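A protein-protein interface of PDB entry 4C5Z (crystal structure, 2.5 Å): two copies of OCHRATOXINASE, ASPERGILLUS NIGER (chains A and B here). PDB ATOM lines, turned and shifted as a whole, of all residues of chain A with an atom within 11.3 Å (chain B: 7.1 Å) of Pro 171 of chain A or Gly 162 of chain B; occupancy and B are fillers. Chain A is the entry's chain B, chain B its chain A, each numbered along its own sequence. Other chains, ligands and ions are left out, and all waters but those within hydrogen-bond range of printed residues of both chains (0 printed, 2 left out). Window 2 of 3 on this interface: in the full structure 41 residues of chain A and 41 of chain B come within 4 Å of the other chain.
O of Leu 86 of chain B is in hydrogen-bond range of OH of Tyr 173 of chain A, 2.7 Å away.
The guanidinium group of Arg 170 of chain B sits at hydrogen-bond distance from the backbone carbonyl oxygen of Pro 171 of chain A, 3.2 Å away.
The backbone carbonyl oxygen (O) of Pro 171 of chain B sits at hydrogen-bond distance from the guanidinium group (NH1) of Arg 170 of chain A (3.3 Å).
The backbone carbonyl oxygen of Glu 159 of chain B is in hydrogen-bond range of the side-chain hydroxyl of Ser 163 of chain B (3.4 Å).
NH2 of Arg 170 of chain B lies within hydrogen-bond range of O of Gly 162 of chain B.
NH2 of Arg 170 of chain B is in hydrogen-bond range of O of Ser 163 of chain B.
NH1 of Arg 170 of chain B is in hydrogen-bond range of O of Gly 172 of chain B (3.4 Å).
O of Gly 162 of chain A sits at hydrogen-bond distance from NH2 of Arg 170 of chain A (3.1 Å).
The guanidinium group (NH2) of Arg 170 of chain A is in hydrogen-bond range of the backbone carbonyl oxygen (O) of Ser 163 of chain A, 3.1 Å away.
Gly 162 of chain A touches Pro 171 of chain B.
OG of Ser 163 of chain A touches CB of Pro 171 of chain B, 3.8 Å away.
NH1 of Arg 170 of chain A touches CA of Gly 172 of chain B, at 3.7 Å.
Pro 171 of chain A touches Gly 162 of chain B (CG to O, 3.4 Å).
CB of Pro 171 of chain A touches OG of Ser 163 of chain B, at 3.8 Å.
CA of Gly 172 of chain A touches NH1 of Arg 170 of chain B (3.7 Å).
Gly 172 of chain B touches Gly 172 of chain A (CA to O, 3.5 Å).
Tyr 164 of chain A touches none of the printed residues of chain B.
Printed residues of chain B within 4 Å of Arg 170 of chain A: Pro 171 and Gly 172.
Of the printed residues of chain B, Pro 171 of chain A touches Gly 162, Ser 163 and Arg 170.
Printed residues of chain B within 4 Å of Gly 172 of chain A: Arg 170 (3.7 Å) and Gly 172 (3.5 Å).
Of the printed residues of chain A, Leu 86 of chain B touches Tyr 173 (2.7 Å).
No residue of chain A comes within 4 Å of Gly 158 of chain B.
No residue of chain A comes within 4 Å of Val 160 of chain B.
No residue of chain A comes within 4 Å of Leu 161 of chain B.
Of chain A, only Pro 171 (3.4 Å) comes within 4 Å of Gly 162 of chain B.
Of the printed residues of chain A, Ser 163 of chain B touches Pro 171 (3.8 Å).
No residue of chain A comes within 4 Å of Gly 165 of chain B.
Of the 17 printed residues of chain B, 6 touch a printed residue of chain A.
Hydrophobic or aromatic side chains of chain B that line the printed part of chain A: Pro 171.
Among the printed residues, 10 pairs touch across the chains.
Among the printed residues, no Asp or Glu carboxylate lies within 4 Å of a Lys or Arg side-chain nitrogen of the other chain.
Gly 162 of chain A touches Pro 171 of chain B, and with the chains exchanged Pro 171 of chain A touches Gly 162 of chain B.
Arg 170 of chain A touches Pro 171 of chain B, and with the chains exchanged Pro 171 of chain A touches Arg 170 of chain B.
Arg 170 of chain A touches Gly 172 of chain B, and with the chains exchanged Gly 172 of chain A touches Arg 170 of chain B.
Gly 172 of chain A touches its own counterpart, Gly 172 of chain B.
Positions printed for both chains: 161, 162, 163, 164, 165, 167, 168, 170, 171, 172, 173 and 174.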
ATOM      1  N   LEU A 161      14.901   7.994  15.611  1.00  0.00           N
ATOM      2  CA  LEU A 161      14.215   9.021  16.412  1.00  0.00           C
ATOM      3  C   LEU A 161      12.870   8.547  16.950  1.00  0.00           C
ATOM      4  O   LEU A 161      12.439   8.998  17.994  1.00  0.00           O
ATOM      5  CB  LEU A 161      14.047  10.321  15.659  1.00  0.00           C
ATOM      6  CG  LEU A 161      15.276  11.231  15.740  1.00  0.00           C
ATOM      7  CD1 LEU A 161      16.316  10.778  14.709  1.00  0.00           C
ATOM      8  CD2 LEU A 161      14.878  12.683  15.490  1.00  0.00           C
ATOM      9  N   GLY A 162      12.217   7.618  16.265  1.00  0.00           N
ATOM     10  CA  GLY A 162      11.008   7.031  16.838  1.00  0.00           C
ATOM     11  C   GLY A 162      11.312   6.321  18.150  1.00  0.00           C
ATOM     12  O   GLY A 162      10.541   6.384  19.118  1.00  0.00           O
ATOM     13  N   SER A 163      12.448   5.640  18.182  1.00  0.00           N
ATOM     14  CA  SER A 163      12.840   4.885  19.334  1.00  0.00           C
ATOM     15  C   SER A 163      13.373   5.782  20.424  1.00  0.00           C
ATOM     16  O   SER A 163      13.065   5.565  21.552  1.00  0.00           O
ATOM     17  CB  SER A 163      13.919   3.854  18.972  1.00  0.00           C
ATOM     18  OG  SER A 163      13.349   2.700  18.394  1.00  0.00           O
ATOM     19  N   TYR A 164      14.163   6.790  20.067  1.00  0.00           N
ATOM     20  CA  TYR A 164      15.025   7.480  21.010  1.00  0.00           C
ATOM     21  C   TYR A 164      14.906   9.014  21.053  1.00  0.00           C
ATOM     22  O   TYR A 164      15.682   9.685  21.753  1.00  0.00           O
ATOM     23  CB  TYR A 164      16.476   7.127  20.659  1.00  0.00           C
ATOM     24  CG  TYR A 164      16.828   5.660  20.758  1.00  0.00           C
ATOM     25  CD1 TYR A 164      16.449   4.907  21.872  1.00  0.00           C
ATOM     26  CD2 TYR A 164      17.582   5.034  19.778  1.00  0.00           C
ATOM     27  CE1 TYR A 164      16.790   3.576  21.993  1.00  0.00           C
ATOM     28  CE2 TYR A 164      17.928   3.694  19.893  1.00  0.00           C
ATOM     29  CZ  TYR A 164      17.529   2.971  21.000  1.00  0.00           C
ATOM     30  OH  TYR A 164      17.839   1.645  21.153  1.00  0.00           O
ATOM     31  N   GLY A 165      13.953   9.563  20.307  1.00  0.00           N
ATOM     32  CA  GLY A 165      13.727  11.001  20.289  1.00  0.00           C
ATOM     33  C   GLY A 165      12.881  11.438  21.475  1.00  0.00           C
ATOM     34  O   GLY A 165      12.263  10.588  22.142  1.00  0.00           O
ATOM     35  N   MET A 167      10.313  13.692  21.256  1.00  0.00           N
ATOM     36  CA  MET A 167       8.959  14.008  20.779  1.00  0.00           C
ATOM     37  C   MET A 167       8.159  12.728  20.756  1.00  0.00           C
ATOM     38  O   MET A 167       8.726  11.625  20.813  1.00  0.00           O
ATOM     39  CB  MET A 167       9.002  14.528  19.329  1.00  0.00           C
ATOM     40  CG  MET A 167       9.330  13.454  18.257  1.00  0.00           C
ATOM     41  SD  MET A 167      11.055  12.825  18.221  1.00  0.00           S
ATOM     42  CE  MET A 167      11.817  14.361  17.636  1.00  0.00           C
ATOM     43  N   ASN A 168       6.848  12.884  20.581  1.00  0.00           N
ATOM     44  CA  ASN A 168       5.959  11.747  20.285  1.00  0.00           C
ATOM     45  C   ASN A 168       5.913  10.649  21.338  1.00  0.00           C
ATOM     46  O   ASN A 168       6.235   9.501  21.083  1.00  0.00           O
ATOM     47  CB  ASN A 168       6.266  11.206  18.895  1.00  0.00           C
ATOM     48  CG  ASN A 168       5.750  12.122  17.807  1.00  0.00           C
ATOM     49  OD1 ASN A 168       4.881  12.980  18.022  1.00  0.00           O
ATOM     50  ND2 ASN A 168       6.268  11.941  16.628  1.00  0.00           N
ATOM     51  N   PRO A 169       5.504  11.017  22.542  1.00  0.00           N
ATOM     52  CA  PRO A 169       5.380  10.056  23.615  1.00  0.00           C
ATOM     53  C   PRO A 169       4.379   8.978  23.254  1.00  0.00           C
ATOM     54  O   PRO A 169       3.420   9.252  22.577  1.00  0.00           O
ATOM     55  CB  PRO A 169       4.862  10.898  24.790  1.00  0.00           C
ATOM     56  CG  PRO A 169       4.272  12.117  24.157  1.00  0.00           C
ATOM     57  CD  PRO A 169       5.117  12.377  22.960  1.00  0.00           C
ATOM     58  N   ARG A 170       4.613   7.770  23.724  1.00  0.00           N
ATOM     59  CA  ARG A 170       3.869   6.621  23.272  1.00  0.00           C
ATOM     60  C   ARG A 170       4.087   5.490  24.267  1.00  0.00           C
ATOM     61  O   ARG A 170       5.011   5.543  25.079  1.00  0.00           O
ATOM     62  CB  ARG A 170       4.407   6.171  21.919  1.00  0.00           C
ATOM     63  CG  ARG A 170       5.928   6.046  21.932  1.00  0.00           C
ATOM     64  CD  ARG A 170       6.525   5.188  20.793  1.00  0.00           C
ATOM     65  NE  ARG A 170       8.002   5.216  20.824  1.00  0.00           N
ATOM     66  CZ  ARG A 170       8.750   4.581  21.735  1.00  0.00           C
ATOM     67  NH1 ARG A 170       8.198   3.819  22.684  1.00  0.00           N
ATOM     68  NH2 ARG A 170      10.062   4.681  21.683  1.00  0.00           N
ATOM     69  N   PRO A 171       3.254   4.447  24.181  1.00  0.00           N
ATOM     70  CA  PRO A 171       3.510   3.275  24.989  1.00  0.00           C
ATOM     71  C   PRO A 171       4.873   2.675  24.616  1.00  0.00           C
ATOM     72  O   PRO A 171       5.360   2.924  23.514  1.00  0.00           O
ATOM     73  CB  PRO A 171       2.354   2.309  24.628  1.00  0.00           C
ATOM     74  CG  PRO A 171       1.321   3.124  23.951  1.00  0.00           C
ATOM     75  CD  PRO A 171       2.014   4.362  23.404  1.00  0.00           C
ATOM     76  N   GLY A 172       5.485   1.901  25.517  1.00  0.00           N
ATOM     77  CA  GLY A 172       6.717   1.169  25.170  1.00  0.00           C
ATOM     78  C   GLY A 172       7.987   1.727  25.798  1.00  0.00           C
ATOM     79  O   GLY A 172       9.042   1.810  25.159  1.00  0.00           O
ATOM     80  N   TYR A 173       7.882   2.107  27.067  1.00  0.00           N
ATOM     81  CA  TYR A 173       9.034   2.596  27.834  1.00  0.00           C
ATOM     82  C   TYR A 173       9.752   3.706  27.098  1.00  0.00           C
ATOM     83  O   TYR A 173      10.957   3.757  27.029  1.00  0.00           O
ATOM     84  CB  TYR A 173       9.939   1.394  28.205  1.00  0.00           C
ATOM     85  CG  TYR A 173       9.128   0.288  28.895  1.00  0.00           C
ATOM     86  CD1 TYR A 173       8.618   0.479  30.185  1.00  0.00           C
ATOM     87  CD2 TYR A 173       8.824  -0.906  28.245  1.00  0.00           C
ATOM     88  CE1 TYR A 173       7.852  -0.484  30.806  1.00  0.00           C
ATOM     89  CE2 TYR A 173       8.053  -1.894  28.857  1.00  0.00           C
ATOM     90  CZ  TYR A 173       7.573  -1.679  30.138  1.00  0.00           C
ATOM     91  OH  TYR A 173       6.801  -2.651  30.752  1.00  0.00           O
ATOM     92  N   TRP A 174       8.960   4.600  26.543  1.00  0.00           N
ATOM     93  CA  TRP A 174       9.454   5.837  25.899  1.00  0.00           C
ATOM     94  C   TRP A 174      10.368   6.601  26.846  1.00  0.00           C
ATOM     95  O   TRP A 174      10.107   6.689  28.028  1.00  0.00           O
ATOM     96  CB  TRP A 174       8.256   6.718  25.580  1.00  0.00           C
ATOM     97  CG  TRP A 174       8.545   7.898  24.752  1.00  0.00           C
ATOM     98  CD1 TRP A 174       8.769   7.918  23.418  1.00  0.00           C
ATOM     99  CD2 TRP A 174       8.606   9.274  25.195  1.00  0.00           C
ATOM    100  NE1 TRP A 174       8.972   9.210  22.989  1.00  0.00           N
ATOM    101  CE2 TRP A 174       8.889  10.058  24.058  1.00  0.00           C
ATOM    102  CE3 TRP A 174       8.440   9.911  26.438  1.00  0.00           C
ATOM    103  CZ2 TRP A 174       9.036  11.439  24.118  1.00  0.00           C
ATOM    104  CZ3 TRP A 174       8.588  11.309  26.494  1.00  0.00           C
ATOM    105  CH2 TRP A 174       8.882  12.049  25.342  1.00  0.00           C
ATOM    106  N   GLY A 175      11.458   7.119  26.323  1.00  0.00           N
ATOM    107  CA  GLY A 175      12.403   7.904  27.088  1.00  0.00           C
ATOM    108  C   GLY A 175      13.309   7.105  28.004  1.00  0.00           C
ATOM    109  O   GLY A 175      13.961   7.694  28.877  1.00  0.00           O
ATOM    110  N   ALA A 176      13.382   5.788  27.808  1.00  0.00           N
ATOM    111  CA  ALA A 176      14.155   4.943  28.711  1.00  0.00           C
ATOM    112  C   ALA A 176      15.025   3.903  27.984  1.00  0.00           C
ATOM    113  O   ALA A 176      14.869   2.716  28.193  1.00  0.00           O
ATOM    114  CB  ALA A 176      13.199   4.253  29.665  1.00  0.00           C
ATOM    115  N   GLY A 177      15.910   4.355  27.104  1.00  0.00           N
ATOM    116  CA  GLY A 177      16.785   3.483  26.330  1.00  0.00           C
ATOM    117  C   GLY A 177      18.238   3.894  26.520  1.00  0.00           C
ATOM    118  O   GLY A 177      18.532   4.778  27.319  1.00  0.00           O
ATOM    119  N   LEU B  86       3.202  -3.529  33.542  1.00  0.00           N
ATOM    120  CA  LEU B  86       3.359  -2.432  32.570  1.00  0.00           C
ATOM    121  C   LEU B  86       4.419  -1.401  32.976  1.00  0.00           C
ATOM    122  O   LEU B  86       5.181  -0.933  32.145  1.00  0.00           O
ATOM    123  CB  LEU B  86       1.998  -1.758  32.320  1.00  0.00           C
ATOM    124  CG  LEU B  86       1.892  -0.497  31.459  1.00  0.00           C
ATOM    125  CD1 LEU B  86       0.508  -0.419  30.851  1.00  0.00           C
ATOM    126  CD2 LEU B  86       2.227   0.790  32.238  1.00  0.00           C
ATOM    127  N   ALA B 157      -8.487   2.074  29.419  1.00  0.00           N
ATOM    128  CA  ALA B 157      -8.361   1.098  28.327  1.00  0.00           C
ATOM    129  C   ALA B 157      -7.327   1.483  27.270  1.00  0.00           C
ATOM    130  O   ALA B 157      -6.649   0.625  26.748  1.00  0.00           O
ATOM    131  CB  ALA B 157      -9.711   0.905  27.668  1.00  0.00           C
ATOM    132  N   GLY B 158      -7.195   2.778  26.959  1.00  0.00           N
ATOM    133  CA  GLY B 158      -6.265   3.203  25.936  1.00  0.00           C
ATOM    134  C   GLY B 158      -4.818   2.906  26.298  1.00  0.00           C
ATOM    135  O   GLY B 158      -4.023   2.534  25.450  1.00  0.00           O
ATOM    136  N   GLU B 159      -4.474   3.047  27.563  1.00  0.00           N
ATOM    137  CA  GLU B 159      -3.095   2.829  28.011  1.00  0.00           C
ATOM    138  C   GLU B 159      -2.751   1.371  27.889  1.00  0.00           C
ATOM    139  O   GLU B 159      -1.652   0.995  27.479  1.00  0.00           O
ATOM    140  CB  GLU B 159      -2.904   3.303  29.460  1.00  0.00           C
ATOM    141  CG  GLU B 159      -2.789   4.816  29.634  1.00  0.00           C
ATOM    142  CD  GLU B 159      -4.085   5.611  29.425  1.00  0.00           C
ATOM    143  OE1 GLU B 159      -5.163   5.011  29.334  1.00  0.00           O
ATOM    144  OE2 GLU B 159      -4.046   6.870  29.364  1.00  0.00           O
ATOM    145  N   VAL B 160      -3.731   0.534  28.174  1.00  0.00           N
ATOM    146  CA  VAL B 160      -3.506  -0.899  28.164  1.00  0.00           C
ATOM    147  C   VAL B 160      -3.405  -1.446  26.746  1.00  0.00           C
ATOM    148  O   VAL B 160      -2.484  -2.191  26.448  1.00  0.00           O
ATOM    149  CB  VAL B 160      -4.582  -1.649  28.968  1.00  0.00           C
ATOM    150  CG1 VAL B 160      -4.323  -3.156  28.940  1.00  0.00           C
ATOM    151  CG2 VAL B 160      -4.603  -1.118  30.398  1.00  0.00           C
ATOM    152  N   LEU B 161      -4.346  -1.103  25.879  1.00  0.00           N
ATOM    153  CA  LEU B 161      -4.257  -1.562  24.498  1.00  0.00           C
ATOM    154  C   LEU B 161      -3.137  -0.873  23.738  1.00  0.00           C
ATOM    155  O   LEU B 161      -2.588  -1.443  22.801  1.00  0.00           O
ATOM    156  CB  LEU B 161      -5.570  -1.408  23.756  1.00  0.00           C
ATOM    157  CG  LEU B 161      -6.500  -2.605  23.985  1.00  0.00           C
ATOM    158  CD1 LEU B 161      -7.235  -2.440  25.326  1.00  0.00           C
ATOM    159  CD2 LEU B 161      -7.486  -2.734  22.828  1.00  0.00           C
ATOM    160  N   GLY B 162      -2.780   0.340  24.131  1.00  0.00           N
ATOM    161  CA  GLY B 162      -1.609   0.953  23.515  1.00  0.00           C
ATOM    162  C   GLY B 162      -0.350   0.122  23.760  1.00  0.00           C
ATOM    163  O   GLY B 162       0.523  -0.011  22.900  1.00  0.00           O
ATOM    164  N   SER B 163      -0.266  -0.409  24.971  1.00  0.00           N
ATOM    165  CA  SER B 163       0.904  -1.114  25.388  1.00  0.00           C
ATOM    166  C   SER B 163       0.883  -2.491  24.822  1.00  0.00           C
ATOM    167  O   SER B 163       1.911  -2.963  24.403  1.00  0.00           O
ATOM    168  CB  SER B 163       0.981  -1.204  26.917  1.00  0.00           C
ATOM    169  OG  SER B 163       1.551  -0.051  27.480  1.00  0.00           O
ATOM    170  N   TYR B 164      -0.278  -3.137  24.806  1.00  0.00           N
ATOM    171  CA  TYR B 164      -0.363  -4.571  24.636  1.00  0.00           C
ATOM    172  C   TYR B 164      -1.300  -5.077  23.531  1.00  0.00           C
ATOM    173  O   TYR B 164      -1.529  -6.284  23.407  1.00  0.00           O
ATOM    174  CB  TYR B 164      -0.822  -5.162  25.967  1.00  0.00           C
ATOM    175  CG  TYR B 164       0.093  -4.922  27.139  1.00  0.00           C
ATOM    176  CD1 TYR B 164       1.460  -5.118  27.042  1.00  0.00           C
ATOM    177  CD2 TYR B 164      -0.407  -4.564  28.365  1.00  0.00           C
ATOM    178  CE1 TYR B 164       2.310  -4.926  28.131  1.00  0.00           C
ATOM    179  CE2 TYR B 164       0.441  -4.370  29.456  1.00  0.00           C
ATOM    180  CZ  TYR B 164       1.798  -4.555  29.328  1.00  0.00           C
ATOM    181  OH  TYR B 164       2.633  -4.409  30.404  1.00  0.00           O
ATOM    182  N   GLY B 165      -1.854  -4.167  22.739  1.00  0.00           N
ATOM    183  CA  GLY B 165      -2.748  -4.521  21.635  1.00  0.00           C
ATOM    184  C   GLY B 165      -1.942  -4.901  20.413  1.00  0.00           C
ATOM    185  O   GLY B 165      -0.730  -4.656  20.368  1.00  0.00           O
ATOM    186  N   MET B 167      -2.765  -3.916  17.235  1.00  0.00           N
ATOM    187  CA  MET B 167      -2.848  -2.822  16.267  1.00  0.00           C
ATOM    188  C   MET B 167      -1.752  -1.826  16.580  1.00  0.00           C
ATOM    189  O   MET B 167      -1.172  -1.847  17.678  1.00  0.00           O
ATOM    190  CB  MET B 167      -4.188  -2.072  16.415  1.00  0.00           C
ATOM    191  CG  MET B 167      -4.331  -1.200  17.686  1.00  0.00           C
ATOM    192  SD  MET B 167      -4.520  -2.086  19.274  1.00  0.00           S
ATOM    193  CE  MET B 167      -6.145  -2.795  18.957  1.00  0.00           C
ATOM    194  N   ASN B 168      -1.553  -0.897  15.657  1.00  0.00           N
ATOM    195  CA  ASN B 168      -0.740   0.279  15.915  1.00  0.00           C
ATOM    196  C   ASN B 168       0.706  -0.035  16.271  1.00  0.00           C
ATOM    197  O   ASN B 168       1.215   0.356  17.319  1.00  0.00           O
ATOM    198  CB  ASN B 168      -1.425   1.191  16.941  1.00  0.00           C
ATOM    199  CG  ASN B 168      -2.607   1.950  16.345  1.00  0.00           C
ATOM    200  OD1 ASN B 168      -2.757   2.085  15.123  1.00  0.00           O
ATOM    201  ND2 ASN B 168      -3.447   2.444  17.197  1.00  0.00           N
ATOM    202  N   ARG B 170       4.661   0.278  16.501  1.00  0.00           N
ATOM    203  CA  ARG B 170       5.396   1.475  16.894  1.00  0.00           C
ATOM    204  C   ARG B 170       6.728   1.088  17.478  1.00  0.00           C
ATOM    205  O   ARG B 170       6.941  -0.070  17.841  1.00  0.00           O
ATOM    206  CB  ARG B 170       4.606   2.199  17.988  1.00  0.00           C
ATOM    207  CG  ARG B 170       4.181   1.254  19.103  1.00  0.00           C
ATOM    208  CD  ARG B 170       3.741   1.940  20.395  1.00  0.00           C
ATOM    209  NE  ARG B 170       3.172   0.901  21.262  1.00  0.00           N
ATOM    210  CZ  ARG B 170       3.900   0.053  21.958  1.00  0.00           C
ATOM    211  NH1 ARG B 170       5.233   0.124  21.961  1.00  0.00           N
ATOM    212  NH2 ARG B 170       3.294  -0.859  22.681  1.00  0.00           N
ATOM    213  N   PRO B 171       7.621   2.073  17.623  1.00  0.00           N
ATOM    214  CA  PRO B 171       8.845   1.808  18.390  1.00  0.00           C
ATOM    215  C   PRO B 171       8.516   1.371  19.847  1.00  0.00           C
ATOM    216  O   PRO B 171       7.434   1.664  20.330  1.00  0.00           O
ATOM    217  CB  PRO B 171       9.602   3.153  18.358  1.00  0.00           C
ATOM    218  CG  PRO B 171       8.957   3.978  17.283  1.00  0.00           C
ATOM    219  CD  PRO B 171       7.554   3.442  17.084  1.00  0.00           C
ATOM    220  N   GLY B 172       9.421   0.663  20.525  1.00  0.00           N
ATOM    221  CA  GLY B 172       9.224   0.341  21.948  1.00  0.00           C
ATOM    222  C   GLY B 172       8.866  -1.115  22.230  1.00  0.00           C
ATOM    223  O   GLY B 172       8.026  -1.435  23.103  1.00  0.00           O
ATOM    224  N   TYR B 173       9.513  -2.003  21.488  1.00  0.00           N
ATOM    225  CA  TYR B 173       9.380  -3.423  21.706  1.00  0.00           C
ATOM    226  C   TYR B 173       7.930  -3.807  21.694  1.00  0.00           C
ATOM    227  O   TYR B 173       7.474  -4.609  22.486  1.00  0.00           O
ATOM    228  CB  TYR B 173      10.128  -3.828  22.986  1.00  0.00           C
ATOM    229  CG  TYR B 173      11.585  -3.369  22.930  1.00  0.00           C
ATOM    230  CD1 TYR B 173      12.476  -3.952  22.040  1.00  0.00           C
ATOM    231  CD2 TYR B 173      12.045  -2.308  23.714  1.00  0.00           C
ATOM    232  CE1 TYR B 173      13.787  -3.527  21.960  1.00  0.00           C
ATOM    233  CE2 TYR B 173      13.372  -1.872  23.639  1.00  0.00           C
ATOM    234  CZ  TYR B 173      14.237  -2.490  22.770  1.00  0.00           C
ATOM    235  OH  TYR B 173      15.558  -2.077  22.680  1.00  0.00           O
ATOM    236  N   TRP B 174       7.230  -3.249  20.719  1.00  0.00           N
ATOM    237  CA  TRP B 174       5.847  -3.617  20.427  1.00  0.00           C
ATOM    238  C   TRP B 174       5.713  -5.127  20.304  1.00  0.00           C
ATOM    239  O   TRP B 174       6.510  -5.767  19.646  1.00  0.00           O
ATOM    240  CB  TRP B 174       5.431  -2.967  19.109  1.00  0.00           C
ATOM    241  CG  TRP B 174       4.002  -3.036  18.794  1.00  0.00           C
ATOM    242  CD1 TRP B 174       3.011  -2.300  19.360  1.00  0.00           C
ATOM    243  CD2 TRP B 174       3.364  -3.861  17.795  1.00  0.00           C
ATOM    244  NE1 TRP B 174       1.797  -2.611  18.788  1.00  0.00           N
ATOM    245  CE2 TRP B 174       1.988  -3.560  17.819  1.00  0.00           C
ATOM    246  CE3 TRP B 174       3.828  -4.814  16.882  1.00  0.00           C
ATOM    247  CZ2 TRP B 174       1.092  -4.164  16.987  1.00  0.00           C
ATOM    248  CZ3 TRP B 174       2.934  -5.414  16.053  1.00  0.00           C
ATOM    249  CH2 TRP B 174       1.583  -5.085  16.101  1.00  0.00           C
